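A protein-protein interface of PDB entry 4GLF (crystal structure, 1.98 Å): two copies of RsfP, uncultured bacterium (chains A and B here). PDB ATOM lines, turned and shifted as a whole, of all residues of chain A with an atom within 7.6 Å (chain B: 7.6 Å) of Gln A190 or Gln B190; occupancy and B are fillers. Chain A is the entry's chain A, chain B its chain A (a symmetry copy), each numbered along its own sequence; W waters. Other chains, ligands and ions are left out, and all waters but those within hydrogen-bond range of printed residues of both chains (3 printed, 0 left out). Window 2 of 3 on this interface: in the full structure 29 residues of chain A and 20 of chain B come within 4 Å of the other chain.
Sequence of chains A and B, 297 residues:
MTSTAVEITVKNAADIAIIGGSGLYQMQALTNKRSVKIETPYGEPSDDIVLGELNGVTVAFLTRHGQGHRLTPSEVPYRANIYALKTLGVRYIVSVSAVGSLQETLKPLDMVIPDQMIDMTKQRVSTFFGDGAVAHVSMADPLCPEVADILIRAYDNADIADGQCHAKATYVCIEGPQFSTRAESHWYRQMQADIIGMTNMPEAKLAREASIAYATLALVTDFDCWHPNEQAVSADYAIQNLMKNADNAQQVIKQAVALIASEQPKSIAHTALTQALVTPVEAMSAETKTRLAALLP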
ATOM      1  N   LEU A 102      35.503   1.391  16.621  1.00  0.00           N
ATOM      2  CA  LEU A 102      34.924   1.908  15.367  1.00  0.00           C
ATOM      3  C   LEU A 102      34.608   3.413  15.467  1.00  0.00           C
ATOM      4  O   LEU A 102      33.946   3.952  14.621  1.00  0.00           O
ATOM      5  CB  LEU A 102      33.644   1.141  15.046  1.00  0.00           C
ATOM      6  CG  LEU A 102      33.852  -0.344  14.688  1.00  0.00           C
ATOM      7  CD1 LEU A 102      32.520  -1.101  14.739  1.00  0.00           C
ATOM      8  CD2 LEU A 102      34.598  -0.549  13.320  1.00  0.00           C
ATOM      9  N   GLN A 103      35.088   4.091  16.512  1.00  0.00           N
ATOM     10  CA  GLN A 103      34.584   5.431  16.805  1.00  0.00           C
ATOM     11  C   GLN A 103      35.781   6.274  17.265  1.00  0.00           C
ATOM     12  O   GLN A 103      36.597   5.818  18.107  1.00  0.00           O
ATOM     13  CB  GLN A 103      33.495   5.422  17.908  1.00  0.00           C
ATOM     14  CG  GLN A 103      32.186   4.675  17.573  1.00  0.00           C
ATOM     15  CD  GLN A 103      31.439   5.254  16.362  1.00  0.00           C
ATOM     16  OE1 GLN A 103      31.515   6.451  16.132  1.00  0.00           O
ATOM     17  NE2 GLN A 103      30.752   4.387  15.544  1.00  0.00           N
ATOM     18  N   GLU A 184      34.180  -3.422   5.443  1.00  0.00           N
ATOM     19  CA  GLU A 184      33.388  -4.062   6.477  1.00  0.00           C
ATOM     20  C   GLU A 184      33.391  -3.089   7.673  1.00  0.00           C
ATOM     21  O   GLU A 184      32.356  -2.886   8.280  1.00  0.00           O
ATOM     22  CB  GLU A 184      34.005  -5.461   6.889  1.00  0.00           C
ATOM     23  CG  GLU A 184      33.817  -6.535   5.793  1.00  0.00           C
ATOM     24  CD  GLU A 184      34.742  -7.752   5.929  1.00  0.00           C
ATOM     25  OE1 GLU A 184      35.695  -7.775   6.825  1.00  0.00           O
ATOM     26  OE2 GLU A 184      34.459  -8.730   5.149  1.00  0.00           O
ATOM     27  N   SER A 185      34.528  -2.490   7.979  1.00  0.00           N
ATOM     28  CA  SER A 185      34.593  -1.536   9.084  1.00  0.00           C
ATOM     29  C   SER A 185      33.621  -0.373   8.879  1.00  0.00           C
ATOM     30  O   SER A 185      32.935   0.017   9.828  1.00  0.00           O
ATOM     31  CB  SER A 185      35.989  -0.949   9.205  1.00  0.00           C
ATOM     32  OG  SER A 185      36.789  -1.992   9.646  1.00  0.00           O
ATOM     33  N   HIS A 186      33.561   0.155   7.655  1.00  0.00           N
ATOM     34  CA  HIS A 186      32.612   1.212   7.263  1.00  0.00           C
ATOM     35  C   HIS A 186      31.203   0.709   7.439  1.00  0.00           C
ATOM     36  O   HIS A 186      30.327   1.410   7.974  1.00  0.00           O
ATOM     37  CB  HIS A 186      32.843   1.666   5.815  1.00  0.00           C
ATOM     38  CG  HIS A 186      31.802   2.653   5.312  1.00  0.00           C
ATOM     39  ND1 HIS A 186      30.685   2.262   4.679  1.00  0.00           N
ATOM     40  CD2 HIS A 186      31.725   4.042   5.419  1.00  0.00           C
ATOM     41  CE1 HIS A 186      29.939   3.344   4.364  1.00  0.00           C
ATOM     42  NE2 HIS A 186      30.565   4.430   4.840  1.00  0.00           N
ATOM     43  N   TRP A 187      30.968  -0.523   7.018  1.00  0.00           N
ATOM     44  CA  TRP A 187      29.623  -1.109   7.146  1.00  0.00           C
ATOM     45  C   TRP A 187      29.198  -1.251   8.651  1.00  0.00           C
ATOM     46  O   TRP A 187      28.085  -0.906   9.027  1.00  0.00           O
ATOM     47  CB  TRP A 187      29.651  -2.461   6.478  1.00  0.00           C
ATOM     48  CG  TRP A 187      28.391  -3.254   6.624  1.00  0.00           C
ATOM     49  CD1 TRP A 187      27.080  -2.788   6.655  1.00  0.00           C
ATOM     50  CD2 TRP A 187      28.298  -4.711   6.671  1.00  0.00           C
ATOM     51  NE1 TRP A 187      26.171  -3.859   6.696  1.00  0.00           N
ATOM     52  CE2 TRP A 187      26.857  -5.037   6.716  1.00  0.00           C
ATOM     53  CE3 TRP A 187      29.224  -5.737   6.639  1.00  0.00           C
ATOM     54  CZ2 TRP A 187      26.399  -6.340   6.771  1.00  0.00           C
ATOM     55  CZ3 TRP A 187      28.729  -7.066   6.667  1.00  0.00           C
ATOM     56  CH2 TRP A 187      27.356  -7.338   6.756  1.00  0.00           C
ATOM     57  N   TYR A 188      30.105  -1.686   9.513  1.00  0.00           N
ATOM     58  CA  TYR A 188      29.763  -1.792  10.962  1.00  0.00           C
ATOM     59  C   TYR A 188      29.439  -0.473  11.607  1.00  0.00           C
ATOM     60  O   TYR A 188      28.500  -0.397  12.492  1.00  0.00           O
ATOM     61  CB  TYR A 188      30.886  -2.485  11.726  1.00  0.00           C
ATOM     62  CG  TYR A 188      31.279  -3.817  11.121  1.00  0.00           C
ATOM     63  CD1 TYR A 188      30.302  -4.700  10.597  1.00  0.00           C
ATOM     64  CD2 TYR A 188      32.597  -4.244  11.165  1.00  0.00           C
ATOM     65  CE1 TYR A 188      30.666  -5.936  10.087  1.00  0.00           C
ATOM     66  CE2 TYR A 188      32.984  -5.480  10.640  1.00  0.00           C
ATOM     67  CZ  TYR A 188      31.997  -6.302  10.092  1.00  0.00           C
ATOM     68  OH  TYR A 188      32.359  -7.500   9.570  1.00  0.00           O
ATOM     69  N   ARG A 189      30.240   0.558  11.251  1.00  0.00           N
ATOM     70  CA  ARG A 189      29.927   1.940  11.609  1.00  0.00           C
ATOM     71  C   ARG A 189      28.525   2.375  11.182  1.00  0.00           C
ATOM     72  O   ARG A 189      27.844   3.063  11.948  1.00  0.00           O
ATOM     73  CB  ARG A 189      31.002   2.966  11.122  1.00  0.00           C
ATOM     74  CG  ARG A 189      32.392   2.797  11.752  1.00  0.00           C
ATOM     75  CD  ARG A 189      33.513   3.735  11.228  1.00  0.00           C
ATOM     76  NE  ARG A 189      33.032   5.067  10.890  1.00  0.00           N
ATOM     77  CZ  ARG A 189      32.783   6.073  11.745  1.00  0.00           C
ATOM     78  NH1 ARG A 189      32.971   5.964  13.071  1.00  0.00           N
ATOM     79  NH2 ARG A 189      32.357   7.234  11.252  1.00  0.00           N
ATOM     80  N   GLN A 190      28.110   2.072   9.930  1.00  0.00           N
ATOM     81  CA  GLN A 190      26.762   2.426   9.460  1.00  0.00           C
ATOM     82  C   GLN A 190      25.650   1.637  10.231  1.00  0.00           C
ATOM     83  O   GLN A 190      24.512   2.100  10.368  1.00  0.00           O
ATOM     84  CB  GLN A 190      26.716   2.243   7.907  1.00  0.00           C
ATOM     85  CG  GLN A 190      25.316   2.129   7.334  1.00  0.00           C
ATOM     86  CD  GLN A 190      25.320   1.779   5.835  1.00  0.00           C
ATOM     87  OE1 GLN A 190      26.188   2.234   5.060  1.00  0.00           O
ATOM     88  NE2 GLN A 190      24.330   0.993   5.421  1.00  0.00           N
ATOM     89  N   MET A 191      25.963   0.444  10.716  1.00  0.00           N
ATOM     90  CA  MET A 191      25.039  -0.285  11.559  1.00  0.00           C
ATOM     91  C   MET A 191      25.076   0.254  12.980  1.00  0.00           C
ATOM     92  O   MET A 191      24.410  -0.306  13.838  1.00  0.00           O
ATOM     93  CB  MET A 191      25.388  -1.774  11.661  1.00  0.00           C
ATOM     94  CG  MET A 191      25.480  -2.525  10.360  1.00  0.00           C
ATOM     95  SD  MET A 191      26.488  -4.017  10.475  1.00  0.00           S
ATOM     96  CE  MET A 191      26.117  -4.671  12.035  1.00  0.00           C
ATOM     97  N   GLN A 192      25.838   1.335  13.211  1.00  0.00           N
ATOM     98  CA  GLN A 192      25.991   1.945  14.552  1.00  0.00           C
ATOM     99  C   GLN A 192      26.694   1.041  15.557  1.00  0.00           C
ATOM    100  O   GLN A 192      26.401   1.075  16.767  1.00  0.00           O
ATOM    101  CB  GLN A 192      24.624   2.303  15.173  1.00  0.00           C
ATOM    102  CG  GLN A 192      23.595   2.836  14.201  1.00  0.00           C
ATOM    103  CD  GLN A 192      23.899   4.237  13.775  1.00  0.00           C
ATOM    104  OE1 GLN A 192      23.495   5.185  14.444  1.00  0.00           O
ATOM    105  NE2 GLN A 192      24.579   4.388  12.629  1.00  0.00           N
ATOM    106  N   ALA A 193      27.552   0.157  15.110  1.00  0.00           N
ATOM    107  CA  ALA A 193      28.366  -0.514  16.129  1.00  0.00           C
ATOM    108  C   ALA A 193      29.504   0.434  16.545  1.00  0.00           C
ATOM    109  O   ALA A 193      29.879   1.263  15.769  1.00  0.00           O
ATOM    110  CB  ALA A 193      28.969  -1.770  15.566  1.00  0.00           C
ATOM    111  N   LEU B 102       8.712  -5.787  13.064  1.00  0.00           N
ATOM    112  CA  LEU B 102       9.717  -4.715  13.192  1.00  0.00           C
ATOM    113  C   LEU B 102       9.096  -3.325  12.951  1.00  0.00           C
ATOM    114  O   LEU B 102       9.801  -2.361  12.811  1.00  0.00           O
ATOM    115  CB  LEU B 102      10.840  -4.951  12.185  1.00  0.00           C
ATOM    116  CG  LEU B 102      11.701  -6.200  12.457  1.00  0.00           C
ATOM    117  CD1 LEU B 102      12.545  -6.549  11.225  1.00  0.00           C
ATOM    118  CD2 LEU B 102      12.574  -6.075  13.757  1.00  0.00           C
ATOM    119  N   GLN B 103       7.766  -3.227  12.904  1.00  0.00           N
ATOM    120  CA  GLN B 103       7.142  -2.007  12.398  1.00  0.00           C
ATOM    121  C   GLN B 103       5.909  -1.733  13.269  1.00  0.00           C
ATOM    122  O   GLN B 103       5.108  -2.661  13.551  1.00  0.00           O
ATOM    123  CB  GLN B 103       6.717  -2.137  10.912  1.00  0.00           C
ATOM    124  CG  GLN B 103       7.853  -2.341   9.889  1.00  0.00           C
ATOM    125  CD  GLN B 103       8.865  -1.186   9.853  1.00  0.00           C
ATOM    126  OE1 GLN B 103       8.483  -0.052  10.097  1.00  0.00           O
ATOM    127  NE2 GLN B 103      10.184  -1.482   9.599  1.00  0.00           N
ATOM    128  N   GLU B 184      20.292  -5.645  17.033  1.00  0.00           N
ATOM    129  CA  GLU B 184      20.079  -6.391  15.806  1.00  0.00           C
ATOM    130  C   GLU B 184      18.694  -5.960  15.286  1.00  0.00           C
ATOM    131  O   GLU B 184      18.545  -5.732  14.101  1.00  0.00           O
ATOM    132  CB  GLU B 184      20.122  -7.951  16.069  1.00  0.00           C
ATOM    133  CG  GLU B 184      21.550  -8.461  16.373  1.00  0.00           C
ATOM    134  CD  GLU B 184      21.605  -9.838  17.048  1.00  0.00           C
ATOM    135  OE1 GLU B 184      20.510 -10.434  17.447  1.00  0.00           O
ATOM    136  OE2 GLU B 184      22.777 -10.352  17.123  1.00  0.00           O
ATOM    137  N   SER B 185      17.715  -5.833  16.165  1.00  0.00           N
ATOM    138  CA  SER B 185      16.385  -5.402  15.743  1.00  0.00           C
ATOM    139  C   SER B 185      16.429  -4.035  15.057  1.00  0.00           C
ATOM    140  O   SER B 185      15.782  -3.857  14.022  1.00  0.00           O
ATOM    141  CB  SER B 185      15.454  -5.284  16.937  1.00  0.00           C
ATOM    142  OG  SER B 185      15.239  -6.586  17.365  1.00  0.00           O
ATOM    143  N   HIS B 186      17.191  -3.100  15.625  1.00  0.00           N
ATOM    144  CA  HIS B 186      17.423  -1.765  15.044  1.00  0.00           C
ATOM    145  C   HIS B 186      18.085  -1.914  13.698  1.00  0.00           C
ATOM    146  O   HIS B 186      17.707  -1.256  12.715  1.00  0.00           O
ATOM    147  CB  HIS B 186      18.277  -0.889  15.970  1.00  0.00           C
ATOM    148  CG  HIS B 186      18.664   0.447  15.359  1.00  0.00           C
ATOM    149  ND1 HIS B 186      19.800   0.620  14.666  1.00  0.00           N
ATOM    150  CD2 HIS B 186      17.992   1.669  15.317  1.00  0.00           C
ATOM    151  CE1 HIS B 186      19.876   1.897  14.226  1.00  0.00           C
ATOM    152  NE2 HIS B 186      18.756   2.529  14.605  1.00  0.00           N
ATOM    153  N   TRP B 187      19.066  -2.799  13.629  1.00  0.00           N
ATOM    154  CA  TRP B 187      19.777  -3.020  12.359  1.00  0.00           C
ATOM    155  C   TRP B 187      18.818  -3.588  11.253  1.00  0.00           C
ATOM    156  O   TRP B 187      18.822  -3.129  10.117  1.00  0.00           O
ATOM    157  CB  TRP B 187      20.900  -3.990  12.629  1.00  0.00           C
ATOM    158  CG  TRP B 187      21.655  -4.425  11.414  1.00  0.00           C
ATOM    159  CD1 TRP B 187      21.961  -3.680  10.278  1.00  0.00           C
ATOM    160  CD2 TRP B 187      22.305  -5.719  11.228  1.00  0.00           C
ATOM    161  NE1 TRP B 187      22.779  -4.415   9.405  1.00  0.00           N
ATOM    162  CE2 TRP B 187      23.006  -5.654   9.929  1.00  0.00           C
ATOM    163  CE3 TRP B 187      22.408  -6.865  11.995  1.00  0.00           C
ATOM    164  CZ2 TRP B 187      23.732  -6.719   9.430  1.00  0.00           C
ATOM    165  CZ3 TRP B 187      23.181  -7.934  11.476  1.00  0.00           C
ATOM    166  CH2 TRP B 187      23.796  -7.854  10.217  1.00  0.00           C
ATOM    167  N   TYR B 188      17.955  -4.528  11.605  1.00  0.00           N
ATOM    168  CA  TYR B 188      16.989  -5.066  10.601  1.00  0.00           C
ATOM    169  C   TYR B 188      16.022  -4.040  10.079  1.00  0.00           C
ATOM    170  O   TYR B 188      15.670  -4.052   8.836  1.00  0.00           O
ATOM    171  CB  TYR B 188      16.230  -6.257  11.175  1.00  0.00           C
ATOM    172  CG  TYR B 188      17.143  -7.326  11.736  1.00  0.00           C
ATOM    173  CD1 TYR B 188      18.355  -7.670  11.085  1.00  0.00           C
ATOM    174  CD2 TYR B 188      16.757  -8.066  12.843  1.00  0.00           C
ATOM    175  CE1 TYR B 188      19.162  -8.682  11.580  1.00  0.00           C
ATOM    176  CE2 TYR B 188      17.567  -9.078  13.364  1.00  0.00           C
ATOM    177  CZ  TYR B 188      18.775  -9.356  12.721  1.00  0.00           C
ATOM    178  OH  TYR B 188      19.575 -10.329  13.223  1.00  0.00           O
ATOM    179  N   ARG B 189      15.516  -3.196  11.009  1.00  0.00           N
ATOM    180  CA  ARG B 189      14.743  -2.011  10.640  1.00  0.00           C
ATOM    181  C   ARG B 189      15.465  -1.102   9.645  1.00  0.00           C
ATOM    182  O   ARG B 189      14.829  -0.592   8.718  1.00  0.00           O
ATOM    183  CB  ARG B 189      14.232  -1.195  11.872  1.00  0.00           C
ATOM    184  CG  ARG B 189      13.235  -1.938  12.774  1.00  0.00           C
ATOM    185  CD  ARG B 189      12.774  -1.199  14.058  1.00  0.00           C
ATOM    186  NE  ARG B 189      12.646   0.239  13.876  1.00  0.00           N
ATOM    187  CZ  ARG B 189      11.620   0.890  13.303  1.00  0.00           C
ATOM    188  NH1 ARG B 189      10.537   0.257  12.820  1.00  0.00           N
ATOM    189  NH2 ARG B 189      11.669   2.218  13.232  1.00  0.00           N
ATOM    190  N   GLN B 190      16.766  -0.806   9.869  1.00  0.00           N
ATOM    191  CA  GLN B 190      17.537   0.032   8.939  1.00  0.00           C
ATOM    192  C   GLN B 190      17.732  -0.667   7.550  1.00  0.00           C
ATOM    193  O   GLN B 190      17.884  -0.008   6.516  1.00  0.00           O
ATOM    194  CB  GLN B 190      18.872   0.450   9.637  1.00  0.00           C
ATOM    195  CG  GLN B 190      19.954   0.922   8.684  1.00  0.00           C
ATOM    196  CD  GLN B 190      21.300   1.158   9.392  1.00  0.00           C
ATOM    197  OE1 GLN B 190      21.357   1.623  10.550  1.00  0.00           O
ATOM    198  NE2 GLN B 190      22.387   0.865   8.682  1.00  0.00           N
ATOM    199  N   MET B 191      17.750  -1.991   7.523  1.00  0.00           N
ATOM    200  CA  MET B 191      17.783  -2.712   6.268  1.00  0.00           C
ATOM    201  C   MET B 191      16.396  -2.761   5.644  1.00  0.00           C
ATOM    202  O   MET B 191      16.238  -3.403   4.617  1.00  0.00           O
ATOM    203  CB  MET B 191      18.222  -4.170   6.441  1.00  0.00           C
ATOM    204  CG  MET B 191      19.554  -4.388   7.107  1.00  0.00           C
ATOM    205  SD  MET B 191      19.714  -6.025   7.848  1.00  0.00           S
ATOM    206  CE  MET B 191      18.917  -7.084   6.735  1.00  0.00           C
ATOM    207  N   GLN B 192      15.419  -2.078   6.259  1.00  0.00           N
ATOM    208  CA  GLN B 192      14.017  -2.064   5.780  1.00  0.00           C
ATOM    209  C   GLN B 192      13.332  -3.423   5.858  1.00  0.00           C
ATOM    210  O   GLN B 192      12.475  -3.760   5.021  1.00  0.00           O
ATOM    211  CB  GLN B 192      13.926  -1.617   4.305  1.00  0.00           C
ATOM    212  CG  GLN B 192      14.884  -0.517   3.904  1.00  0.00           C
ATOM    213  CD  GLN B 192      14.473   0.811   4.454  1.00  0.00           C
ATOM    214  OE1 GLN B 192      13.684   1.518   3.832  1.00  0.00           O
ATOM    215  NE2 GLN B 192      15.038   1.190   5.610  1.00  0.00           N
ATOM    216  N   ALA B 193      13.730  -4.271   6.775  1.00  0.00           N
ATOM    217  CA  ALA B 193      12.883  -5.455   6.957  1.00  0.00           C
ATOM    218  C   ALA B 193      11.663  -5.057   7.805  1.00  0.00           C
ATOM    219  O   ALA B 193      11.756  -4.129   8.553  1.00  0.00           O
ATOM    220  CB  ALA B 193      13.644  -6.529   7.685  1.00  0.00           C
HETATM  221  O   HOH W   1      21.485  -0.170  12.848  1.00  0.00           O
HETATM  222  O   HOH W   2      23.331  -2.832   6.889  1.00  0.00           O
HETATM  223  O   HOH W   3      21.842  -1.323  15.655  1.00  0.00           O
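Of the printed residues of chain B, Trp A187 touches Trp B187 (3.8 Å). Gln A190 touches just one residue of chain B: Gln B190 (3.0 Å). Ser B185 touches none of the printed residues of chain A. Printed residues of chain A within 4 Å of Trp B187: Trp A187 and Met A191. Of chain A, only Gln A190 (3.0 Å) comes within 4 Å of Gln B190. Gln B192 touches none of the printed residues of chain A.
CZ2 of Trp A187 touches CZ2 of Trp B187, at 3.8 Å. Met A191 touches Trp B187 (CG to NE1, 3.4 Å). His B186 touches Gln A192 (CE1 to CG, 3.8 Å).
The side-chain sulfur of Met B191 is in hydrogen-bond range of the indole nitrogen of Trp B187 (3.8 Å). The backbone carbonyl oxygen (O) of Gln A190 lies within hydrogen-bond range of the side-chain amide nitrogen (NE2) of Gln A192 (3.2 Å). SD of Met A191 lies within hydrogen-bond range of NE1 of Trp A187 (3.8 Å). O of Gln B190 sits at hydrogen-bond distance from NE2 of Gln B192 (3.2 Å).
Trp B187 touches its own counterpart, Trp A187. Gln A190 touches its own counterpart, Gln B190. Met A191 touches Trp B187, but with the chains exchanged Trp A187 does not touch Met B191 (6.7 Å). Gln A192 touches His B186, but with the chains exchanged His A186 does not touch Gln B192 (15.1 Å). 12 positions are printed for both chains.
O of Gln A190 lies within hydrogen-bond range of NE2 of Gln B190 (3.0 Å).
Water W1 lies within hydrogen-bond range of a ring nitrogen (ND1) of His B186, the side-chain amide oxygen (OE1) of Gln B190 and the backbone carbonyl oxygen (O) of Met A191. Water W3 lies within hydrogen-bond range of a ring nitrogen (ND1) of His B186 (3.0 Å) and the backbone carbonyl oxygen of Met A191 (3.3 Å). Water W2 bridges the indole nitrogen (NE1) of Trp B187 and the indole nitrogen (NE1) of Trp A187.
Hydrophobic or aromatic side chains of chain B within 4 Å of the printed part of chain A: His B186 and Trp B187. Of the 12 printed residues of chain A, 4 touch a printed residue of chain B. Hydrophobic or aromatic side chains of chain A within 4 Å of the printed part of chain B: Trp A187 and Met A191.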
